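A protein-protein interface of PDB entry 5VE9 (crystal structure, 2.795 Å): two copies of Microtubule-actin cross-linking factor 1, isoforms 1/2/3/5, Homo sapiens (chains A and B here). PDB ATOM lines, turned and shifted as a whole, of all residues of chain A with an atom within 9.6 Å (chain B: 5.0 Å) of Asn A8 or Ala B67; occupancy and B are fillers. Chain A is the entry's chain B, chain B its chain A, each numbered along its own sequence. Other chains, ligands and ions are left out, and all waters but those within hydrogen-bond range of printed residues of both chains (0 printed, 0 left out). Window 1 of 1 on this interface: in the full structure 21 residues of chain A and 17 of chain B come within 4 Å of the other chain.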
ATOM      1  N   HIS A   5       4.512  23.008 -14.053  1.00  0.00           N
ATOM      2  CA  HIS A   5       3.225  23.296 -14.680  1.00  0.00           C
ATOM      3  C   HIS A   5       2.879  22.225 -15.706  1.00  0.00           C
ATOM      4  O   HIS A   5       3.702  21.890 -16.559  1.00  0.00           O
ATOM      5  CB  HIS A   5       3.246  24.661 -15.370  1.00  0.00           C
ATOM      6  CG  HIS A   5       2.932  25.809 -14.464  1.00  0.00           C
ATOM      7  ND1 HIS A   5       3.848  26.329 -13.574  1.00  0.00           N
ATOM      8  CD2 HIS A   5       1.807  26.549 -14.322  1.00  0.00           C
ATOM      9  CE1 HIS A   5       3.297  27.337 -12.921  1.00  0.00           C
ATOM     10  NE2 HIS A   5       2.058  27.489 -13.354  1.00  0.00           N
ATOM     11  N   MET A   6       1.662  21.696 -15.631  1.00  0.00           N
ATOM     12  CA  MET A   6       1.199  20.738 -16.626  1.00  0.00           C
ATOM     13  C   MET A   6       1.040  21.454 -17.961  1.00  0.00           C
ATOM     14  O   MET A   6       0.346  22.469 -18.050  1.00  0.00           O
ATOM     15  CB  MET A   6      -0.122  20.097 -16.201  1.00  0.00           C
ATOM     16  CG  MET A   6      -0.446  18.819 -16.950  1.00  0.00           C
ATOM     17  SD  MET A   6       0.733  17.511 -16.571  1.00  0.00           S
ATOM     18  CE  MET A   6       0.156  16.209 -17.642  1.00  0.00           C
ATOM     19  N   ALA A   7       1.688  20.927 -18.996  1.00  0.00           N
ATOM     20  CA  ALA A   7       1.747  21.615 -20.279  1.00  0.00           C
ATOM     21  C   ALA A   7       2.055  20.662 -21.423  1.00  0.00           C
ATOM     22  O   ALA A   7       2.661  19.612 -21.220  1.00  0.00           O
ATOM     23  CB  ALA A   7       2.795  22.716 -20.226  1.00  0.00           C
ATOM     24  N   ASN A   8       1.640  21.043 -22.629  1.00  0.00           N
ATOM     25  CA  ASN A   8       1.974  20.286 -23.827  1.00  0.00           C
ATOM     26  C   ASN A   8       3.475  20.282 -24.073  1.00  0.00           C
ATOM     27  O   ASN A   8       4.122  21.329 -24.035  1.00  0.00           O
ATOM     28  CB  ASN A   8       1.257  20.861 -25.052  1.00  0.00           C
ATOM     29  CG  ASN A   8      -0.240  20.639 -25.011  1.00  0.00           C
ATOM     30  OD1 ASN A   8      -0.736  19.784 -24.275  1.00  0.00           O
ATOM     31  ND2 ASN A   8      -0.972  21.401 -25.815  1.00  0.00           N
ATOM     32  N   PHE A   9       4.021  19.097 -24.317  1.00  0.00           N
ATOM     33  CA  PHE A   9       5.421  18.954 -24.696  1.00  0.00           C
ATOM     34  C   PHE A   9       5.525  18.029 -25.899  1.00  0.00           C
ATOM     35  O   PHE A   9       5.017  16.909 -25.872  1.00  0.00           O
ATOM     36  CB  PHE A   9       6.249  18.412 -23.530  1.00  0.00           C
ATOM     37  CG  PHE A   9       7.725  18.376 -23.805  1.00  0.00           C
ATOM     38  CD1 PHE A   9       8.485  19.533 -23.730  1.00  0.00           C
ATOM     39  CD2 PHE A   9       8.355  17.186 -24.135  1.00  0.00           C
ATOM     40  CE1 PHE A   9       9.843  19.506 -23.981  1.00  0.00           C
ATOM     41  CE2 PHE A   9       9.713  17.151 -24.387  1.00  0.00           C
ATOM     42  CZ  PHE A   9      10.458  18.313 -24.311  1.00  0.00           C
ATOM     43  N   ASP A  10       6.172  18.508 -26.958  1.00  0.00           N
ATOM     44  CA  ASP A  10       6.357  17.707 -28.162  1.00  0.00           C
ATOM     45  C   ASP A  10       7.426  16.645 -27.923  1.00  0.00           C
ATOM     46  O   ASP A  10       8.560  16.758 -28.390  1.00  0.00           O
ATOM     47  CB  ASP A  10       6.734  18.590 -29.352  1.00  0.00           C
ATOM     48  CG  ASP A  10       5.538  19.297 -29.959  1.00  0.00           C
ATOM     49  OD1 ASP A  10       4.449  18.688 -30.037  1.00  0.00           O
ATOM     50  OD2 ASP A  10       5.687  20.469 -30.365  1.00  0.00           O
ATOM     51  N   PHE A  11       7.043  15.611 -27.185  1.00  0.00           N
ATOM     52  CA  PHE A  11       7.952  14.533 -26.817  1.00  0.00           C
ATOM     53  C   PHE A  11       8.389  13.710 -28.027  1.00  0.00           C
ATOM     54  O   PHE A  11       9.549  13.301 -28.123  1.00  0.00           O
ATOM     55  CB  PHE A  11       7.280  13.629 -25.788  1.00  0.00           C
ATOM     56  CG  PHE A  11       8.143  12.496 -25.316  1.00  0.00           C
ATOM     57  CD1 PHE A  11       9.177  12.723 -24.424  1.00  0.00           C
ATOM     58  CD2 PHE A  11       7.914  11.201 -25.755  1.00  0.00           C
ATOM     59  CE1 PHE A  11       9.971  11.683 -23.982  1.00  0.00           C
ATOM     60  CE2 PHE A  11       8.705  10.156 -25.316  1.00  0.00           C
ATOM     61  CZ  PHE A  11       9.734  10.397 -24.428  1.00  0.00           C
ATOM     62  N   ASP A  12       7.450  13.464 -28.938  1.00  0.00           N
ATOM     63  CA  ASP A  12       7.735  12.730 -30.170  1.00  0.00           C
ATOM     64  C   ASP A  12       8.897  13.363 -30.929  1.00  0.00           C
ATOM     65  O   ASP A  12       9.796  12.668 -31.404  1.00  0.00           O
ATOM     66  CB  ASP A  12       6.503  12.686 -31.079  1.00  0.00           C
ATOM     67  CG  ASP A  12       5.424  11.740 -30.576  1.00  0.00           C
ATOM     68  OD1 ASP A  12       5.741  10.808 -29.804  1.00  0.00           O
ATOM     69  OD2 ASP A  12       4.252  11.922 -30.975  1.00  0.00           O
ATOM     70  N   LEU A  63      16.020  22.257 -19.014  1.00  0.00           N
ATOM     71  CA  LEU A  63      14.593  22.525 -18.926  1.00  0.00           C
ATOM     72  C   LEU A  63      13.813  21.514 -19.760  1.00  0.00           C
ATOM     73  O   LEU A  63      12.743  21.054 -19.352  1.00  0.00           O
ATOM     74  CB  LEU A  63      14.287  23.953 -19.388  1.00  0.00           C
ATOM     75  CG  LEU A  63      13.427  24.841 -18.479  1.00  0.00           C
ATOM     76  CD1 LEU A  63      13.840  24.751 -17.012  1.00  0.00           C
ATOM     77  CD2 LEU A  63      13.508  26.283 -18.956  1.00  0.00           C
ATOM     78  N   GLU A  64      14.352  21.165 -20.926  1.00  0.00           N
ATOM     79  CA  GLU A  64      13.769  20.106 -21.742  1.00  0.00           C
ATOM     80  C   GLU A  64      13.854  18.771 -21.010  1.00  0.00           C
ATOM     81  O   GLU A  64      12.943  17.949 -21.096  1.00  0.00           O
ATOM     82  CB  GLU A  64      14.474  19.987 -23.100  1.00  0.00           C
ATOM     83  CG  GLU A  64      14.304  21.183 -24.030  1.00  0.00           C
ATOM     84  CD  GLU A  64      14.891  20.938 -25.413  1.00  0.00           C
ATOM     85  OE1 GLU A  64      15.349  19.808 -25.679  1.00  0.00           O
ATOM     86  OE2 GLU A  64      14.895  21.874 -26.237  1.00  0.00           O
ATOM     87  N   ALA A  67      11.206  17.913 -18.262  1.00  0.00           N
ATOM     88  CA  ALA A  67       9.971  17.472 -18.898  1.00  0.00           C
ATOM     89  C   ALA A  67      10.109  16.067 -19.478  1.00  0.00           C
ATOM     90  O   ALA A  67       9.262  15.205 -19.248  1.00  0.00           O
ATOM     91  CB  ALA A  67       9.566  18.442 -19.986  1.00  0.00           C
ATOM     92  N   VAL A  68      11.170  15.848 -20.250  1.00  0.00           N
ATOM     93  CA  VAL A  68      11.418  14.543 -20.862  1.00  0.00           C
ATOM     94  C   VAL A  68      11.471  13.437 -19.805  1.00  0.00           C
ATOM     95  O   VAL A  68      10.826  12.399 -19.955  1.00  0.00           O
ATOM     96  CB  VAL A  68      12.731  14.544 -21.676  1.00  0.00           C
ATOM     97  CG1 VAL A  68      13.140  13.125 -22.051  1.00  0.00           C
ATOM     98  CG2 VAL A  68      12.572  15.398 -22.929  1.00  0.00           C
ATOM     99  N   ILE A  71       8.131  12.466 -18.580  1.00  0.00           N
ATOM    100  CA  ILE A  71       7.409  11.606 -19.512  1.00  0.00           C
ATOM    101  C   ILE A  71       7.919  10.164 -19.474  1.00  0.00           C
ATOM    102  O   ILE A  71       7.128   9.224 -19.419  1.00  0.00           O
ATOM    103  CB  ILE A  71       7.505  12.139 -20.954  1.00  0.00           C
ATOM    104  CG1 ILE A  71       6.744  13.461 -21.062  1.00  0.00           C
ATOM    105  CG2 ILE A  71       6.948  11.109 -21.938  1.00  0.00           C
ATOM    106  CD1 ILE A  71       6.856  14.146 -22.397  1.00  0.00           C
ATOM    107  N   HIS B   5       1.548  14.364 -26.047  1.00  0.00           N
ATOM    108  CA  HIS B   5       2.261  14.225 -24.782  1.00  0.00           C
ATOM    109  C   HIS B   5       2.204  15.505 -23.957  1.00  0.00           C
ATOM    110  O   HIS B   5       2.111  16.609 -24.498  1.00  0.00           O
ATOM    111  CB  HIS B   5       3.720  13.839 -25.025  1.00  0.00           C
ATOM    112  CG  HIS B   5       3.922  12.381 -25.281  1.00  0.00           C
ATOM    113  ND1 HIS B   5       4.061  11.858 -26.549  1.00  0.00           N
ATOM    114  CD2 HIS B   5       4.001  11.328 -24.430  1.00  0.00           C
ATOM    115  CE1 HIS B   5       4.222  10.550 -26.469  1.00  0.00           C
ATOM    116  NE2 HIS B   5       4.190  10.203 -25.195  1.00  0.00           N
ATOM    117  N   MET B   6       2.267  15.336 -22.641  1.00  0.00           N
ATOM    118  CA  MET B   6       2.236  16.449 -21.703  1.00  0.00           C
ATOM    119  C   MET B   6       3.158  16.143 -20.529  1.00  0.00           C
ATOM    120  O   MET B   6       3.346  14.980 -20.166  1.00  0.00           O
ATOM    121  CB  MET B   6       0.808  16.701 -21.215  1.00  0.00           C
ATOM    122  CG  MET B   6      -0.094  17.387 -22.236  1.00  0.00           C
ATOM    123  SD  MET B   6      -1.860  17.090 -21.986  1.00  0.00           S
ATOM    124  CE  MET B   6      -1.940  16.887 -20.212  1.00  0.00           C
ATOM    125  N   PHE B   9       6.277  21.000 -16.680  1.00  0.00           N
ATOM    126  CA  PHE B   9       7.362  21.865 -17.123  1.00  0.00           C
ATOM    127  C   PHE B   9       7.772  22.817 -16.007  1.00  0.00           C
ATOM    128  O   PHE B   9       6.922  23.415 -15.348  1.00  0.00           O
ATOM    129  CB  PHE B   9       6.945  22.654 -18.364  1.00  0.00           C
ATOM    130  CG  PHE B   9       8.076  23.405 -19.012  1.00  0.00           C
ATOM    131  CD1 PHE B   9       8.973  22.750 -19.838  1.00  0.00           C
ATOM    132  CD2 PHE B   9       8.241  24.764 -18.797  1.00  0.00           C
ATOM    133  CE1 PHE B   9      10.013  23.435 -20.436  1.00  0.00           C
ATOM    134  CE2 PHE B   9       9.280  25.453 -19.394  1.00  0.00           C
ATOM    135  CZ  PHE B   9      10.167  24.787 -20.215  1.00  0.00           C
ATOM    136  N   ARG B  46      -0.181  31.989 -29.861  1.00  0.00           N
ATOM    137  CA  ARG B  46       0.905  31.218 -29.269  1.00  0.00           C
ATOM    138  C   ARG B  46       2.143  31.290 -30.153  1.00  0.00           C
ATOM    139  O   ARG B  46       3.265  31.378 -29.659  1.00  0.00           O
ATOM    140  CB  ARG B  46       0.501  29.758 -29.075  1.00  0.00           C
ATOM    141  CG  ARG B  46      -0.656  29.528 -28.122  1.00  0.00           C
ATOM    142  CD  ARG B  46      -0.776  28.050 -27.781  1.00  0.00           C
ATOM    143  NE  ARG B  46      -2.048  27.710 -27.152  1.00  0.00           N
ATOM    144  CZ  ARG B  46      -2.282  26.569 -26.509  1.00  0.00           C
ATOM    145  NH1 ARG B  46      -1.322  25.661 -26.395  1.00  0.00           N
ATOM    146  NH2 ARG B  46      -3.471  26.342 -25.969  1.00  0.00           N
ATOM    147  N   LEU B  63      11.205  23.529 -28.284  1.00  0.00           N
ATOM    148  CA  LEU B  63      10.624  22.493 -27.435  1.00  0.00           C
ATOM    149  C   LEU B  63      10.182  23.064 -26.096  1.00  0.00           C
ATOM    150  O   LEU B  63       9.133  22.692 -25.570  1.00  0.00           O
ATOM    151  CB  LEU B  63      11.620  21.353 -27.205  1.00  0.00           C
ATOM    152  CG  LEU B  63      11.771  20.299 -28.307  1.00  0.00           C
ATOM    153  CD1 LEU B  63      12.718  19.205 -27.843  1.00  0.00           C
ATOM    154  CD2 LEU B  63      10.428  19.701 -28.709  1.00  0.00           C
ATOM    155  N   GLU B  64      10.988  23.963 -25.540  1.00  0.00           N
ATOM    156  CA  GLU B  64      10.605  24.658 -24.317  1.00  0.00           C
ATOM    157  C   GLU B  64       9.422  25.579 -24.577  1.00  0.00           C
ATOM    158  O   GLU B  64       8.504  25.673 -23.766  1.00  0.00           O
ATOM    159  CB  GLU B  64      11.769  25.480 -23.755  1.00  0.00           C
ATOM    160  CG  GLU B  64      12.960  24.668 -23.293  1.00  0.00           C
ATOM    161  CD  GLU B  64      14.076  25.535 -22.741  1.00  0.00           C
ATOM    162  OE1 GLU B  64      13.933  26.774 -22.757  1.00  0.00           O
ATOM    163  OE2 GLU B  64      15.095  24.977 -22.288  1.00  0.00           O
ATOM    164  N   MET B  65       9.447  26.252 -25.721  1.00  0.00           N
ATOM    165  CA  MET B  65       8.534  27.360 -25.966  1.00  0.00           C
ATOM    166  C   MET B  65       7.106  26.920 -26.280  1.00  0.00           C
ATOM    167  O   MET B  65       6.165  27.685 -26.063  1.00  0.00           O
ATOM    168  CB  MET B  65       9.067  28.232 -27.103  1.00  0.00           C
ATOM    169  CG  MET B  65      10.204  29.159 -26.686  1.00  0.00           C
ATOM    170  SD  MET B  65       9.815  30.183 -25.249  1.00  0.00           S
ATOM    171  CE  MET B  65       8.317  31.000 -25.801  1.00  0.00           C
ATOM    172  N   THR B  66       6.931  25.705 -26.788  1.00  0.00           N
ATOM    173  CA  THR B  66       5.586  25.167 -26.949  1.00  0.00           C
ATOM    174  C   THR B  66       4.989  24.934 -25.567  1.00  0.00           C
ATOM    175  O   THR B  66       3.788  25.101 -25.361  1.00  0.00           O
ATOM    176  CB  THR B  66       5.561  23.849 -27.757  1.00  0.00           C
ATOM    177  OG1 THR B  66       6.525  22.932 -27.225  1.00  0.00           O
ATOM    178  CG2 THR B  66       5.862  24.111 -29.222  1.00  0.00           C
ATOM    179  N   ALA B  67       5.841  24.560 -24.618  1.00  0.00           N
ATOM    180  CA  ALA B  67       5.400  24.328 -23.250  1.00  0.00           C
ATOM    181  C   ALA B  67       5.046  25.636 -22.539  1.00  0.00           C
ATOM    182  O   ALA B  67       4.001  25.727 -21.893  1.00  0.00           O
ATOM    183  CB  ALA B  67       6.466  23.576 -22.461  1.00  0.00           C
ATOM    184  N   VAL B  68       5.906  26.648 -22.645  1.00  0.00           N
ATOM    185  CA  VAL B  68       5.643  27.909 -21.953  1.00  0.00           C
ATOM    186  C   VAL B  68       4.452  28.619 -22.600  1.00  0.00           C
ATOM    187  O   VAL B  68       3.615  29.192 -21.903  1.00  0.00           O
ATOM    188  CB  VAL B  68       6.880  28.858 -21.936  1.00  0.00           C
ATOM    189  CG1 VAL B  68       8.146  28.096 -21.568  1.00  0.00           C
ATOM    190  CG2 VAL B  68       7.058  29.571 -23.266  1.00  0.00           C
ATOM    191  N   ALA B  69       4.366  28.563 -23.926  1.00  0.00           N
ATOM    192  CA  ALA B  69       3.246  29.171 -24.638  1.00  0.00           C
ATOM    193  C   ALA B  69       1.950  28.462 -24.266  1.00  0.00           C
ATOM    194  O   ALA B  69       0.880  29.068 -24.261  1.00  0.00           O
ATOM    195  CB  ALA B  69       3.468  29.125 -26.147  1.00  0.00           C
ATOM    196  N   ASP B  70       2.052  27.173 -23.954  1.00  0.00           N
ATOM    197  CA  ASP B  70       0.898  26.410 -23.496  1.00  0.00           C
ATOM    198  C   ASP B  70       0.462  26.919 -22.125  1.00  0.00           C
ATOM    199  O   ASP B  70      -0.729  27.078 -21.856  1.00  0.00           O
ATOM    200  CB  ASP B  70       1.221  24.915 -23.428  1.00  0.00           C
ATOM    201  CG  ASP B  70      -0.009  24.063 -23.198  1.00  0.00           C
ATOM    202  OD1 ASP B  70      -0.756  23.828 -24.170  1.00  0.00           O
ATOM    203  OD2 ASP B  70      -0.225  23.623 -22.050  1.00  0.00           O
ATOM    204  N   ILE B  71       1.442  27.180 -21.265  1.00  0.00           N
ATOM    205  CA  ILE B  71       1.181  27.621 -19.896  1.00  0.00           C
ATOM    206  C   ILE B  71       0.621  29.045 -19.850  1.00  0.00           C
ATOM    207  O   ILE B  71      -0.256  29.349 -19.039  1.00  0.00           O
ATOM    208  CB  ILE B  71       2.463  27.546 -19.040  1.00  0.00           C
ATOM    209  CG1 ILE B  71       2.859  26.083 -18.839  1.00  0.00           C
ATOM    210  CG2 ILE B  71       2.251  28.227 -17.691  1.00  0.00           C
ATOM    211  CD1 ILE B  71       4.259  25.883 -18.313  1.00  0.00           C
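Met B6 touches Met A6 (CE to CE, 3.4 Å). Ala A7 touches Asp B70 (CA to OD2, 3.3 Å). Asn A8 touches His B5. Asn A8 touches Ala B67. Phe A9 touches Leu B63. O of Asp A10 touches CD2 of Leu B63, at 3.5 Å. Glu B64 touches Leu A63. Glu A64 touches Leu B63. Glu A64 touches Glu B64 (CG to CG, 3.8 Å). CG1 of Ile A71 touches O of Met B6 (3.8 Å).
NH1 of Arg B46 lies within salt-bridge range of OD1 of Asp B70 (2.9 Å). The side-chain hydroxyl of Thr B66 sits at hydrogen-bond distance from the backbone carbonyl oxygen of Leu B63 (3.1 Å).
Of the printed residues of chain B, Asn A8 touches His B5 (3.7 Å), Met B6 (3.2 Å), Ala B67 (3.4 Å) and Asp B70 (2.9 Å). Ala B67 touches two residues of chain A. No residue of chain A comes within 4 Å of Val B68. Asp B70 touches just these residues of chain A: Ala A7 (3.3 Å) and Asn A8 (2.9 Å). Of the printed residues of chain B, Phe A11 touches His B5 (3.6 Å). Printed residues of chain A within 4 Å of His B5: Asn A8, Phe A9, Phe A11, Asp A12 and Ile A71. Of the printed residues of chain B, Phe A9 touches His B5 and Leu B63. Of the printed residues of chain B, Ile A71 touches His B5 and Met B6. Printed residues of chain B within 4 Å of Asp A12: His B5. Met B65 touches none of the printed residues of chain A. The nearest printed residue of chain B that does not touch Asn A8 is Thr B66 (4.01 Å). The nearest residue of chain A that does not touch Ala B67 is Phe A9 (4.7 Å). The nearest printed residue of chain B that does not touch Glu A64 is Phe B9 (4.9 Å).
His A5 touches Phe B9, and with the chains exchanged Phe A9 touches His B5. His A5 touches Ile B71, and with the chains exchanged Ile A71 touches His B5. Leu A63 touches Glu B64, and with the chains exchanged Glu A64 touches Leu B63. Ile A71 touches Met B6, but with the chains exchanged Met A6 does not touch Ile B71 (4.5 Å). Positions printed for both chains: 5, 6, 9, 63, 64, 67, 68 and 71.
The side-chain amide nitrogen of Asn A8 lies within hydrogen-bond range of the side-chain carboxylate of Asp B70, 2.9 Å away. N of Phe A9 is in hydrogen-bond range of O of His B5. The backbone carbonyl oxygen (O) of His A5 is in hydrogen-bond range of the backbone NH (N) of Phe B9 (2.7 Å). The side-chain sulfur of Met B6 sits close to the side-chain amide oxygen of Asn A8, at 3.7 Å.
Of the 13 printed residues of chain B, 9 touch a printed residue of chain A. Hydrophobic or aromatic side chains of chain B that line the printed part of chain A: His B5, Met B6, Phe B9, Leu B63, Ala B67 and Ile B71. Printed residues of chain A that touch a printed residue of chain B: His A5, Met A6, Ala A7, Asn A8, Phe A9, Asp A10, Phe A11, Asp A12, Leu A63, Glu A64 and Ile A71. Hydrophobic or aromatic side chains of chain A that line the printed part of chain B: His A5, Met A6, Ala A7, Phe A9, Phe A11, Leu A63 and Ile A71. Among the printed residues, 23 pairs touch across the chains.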
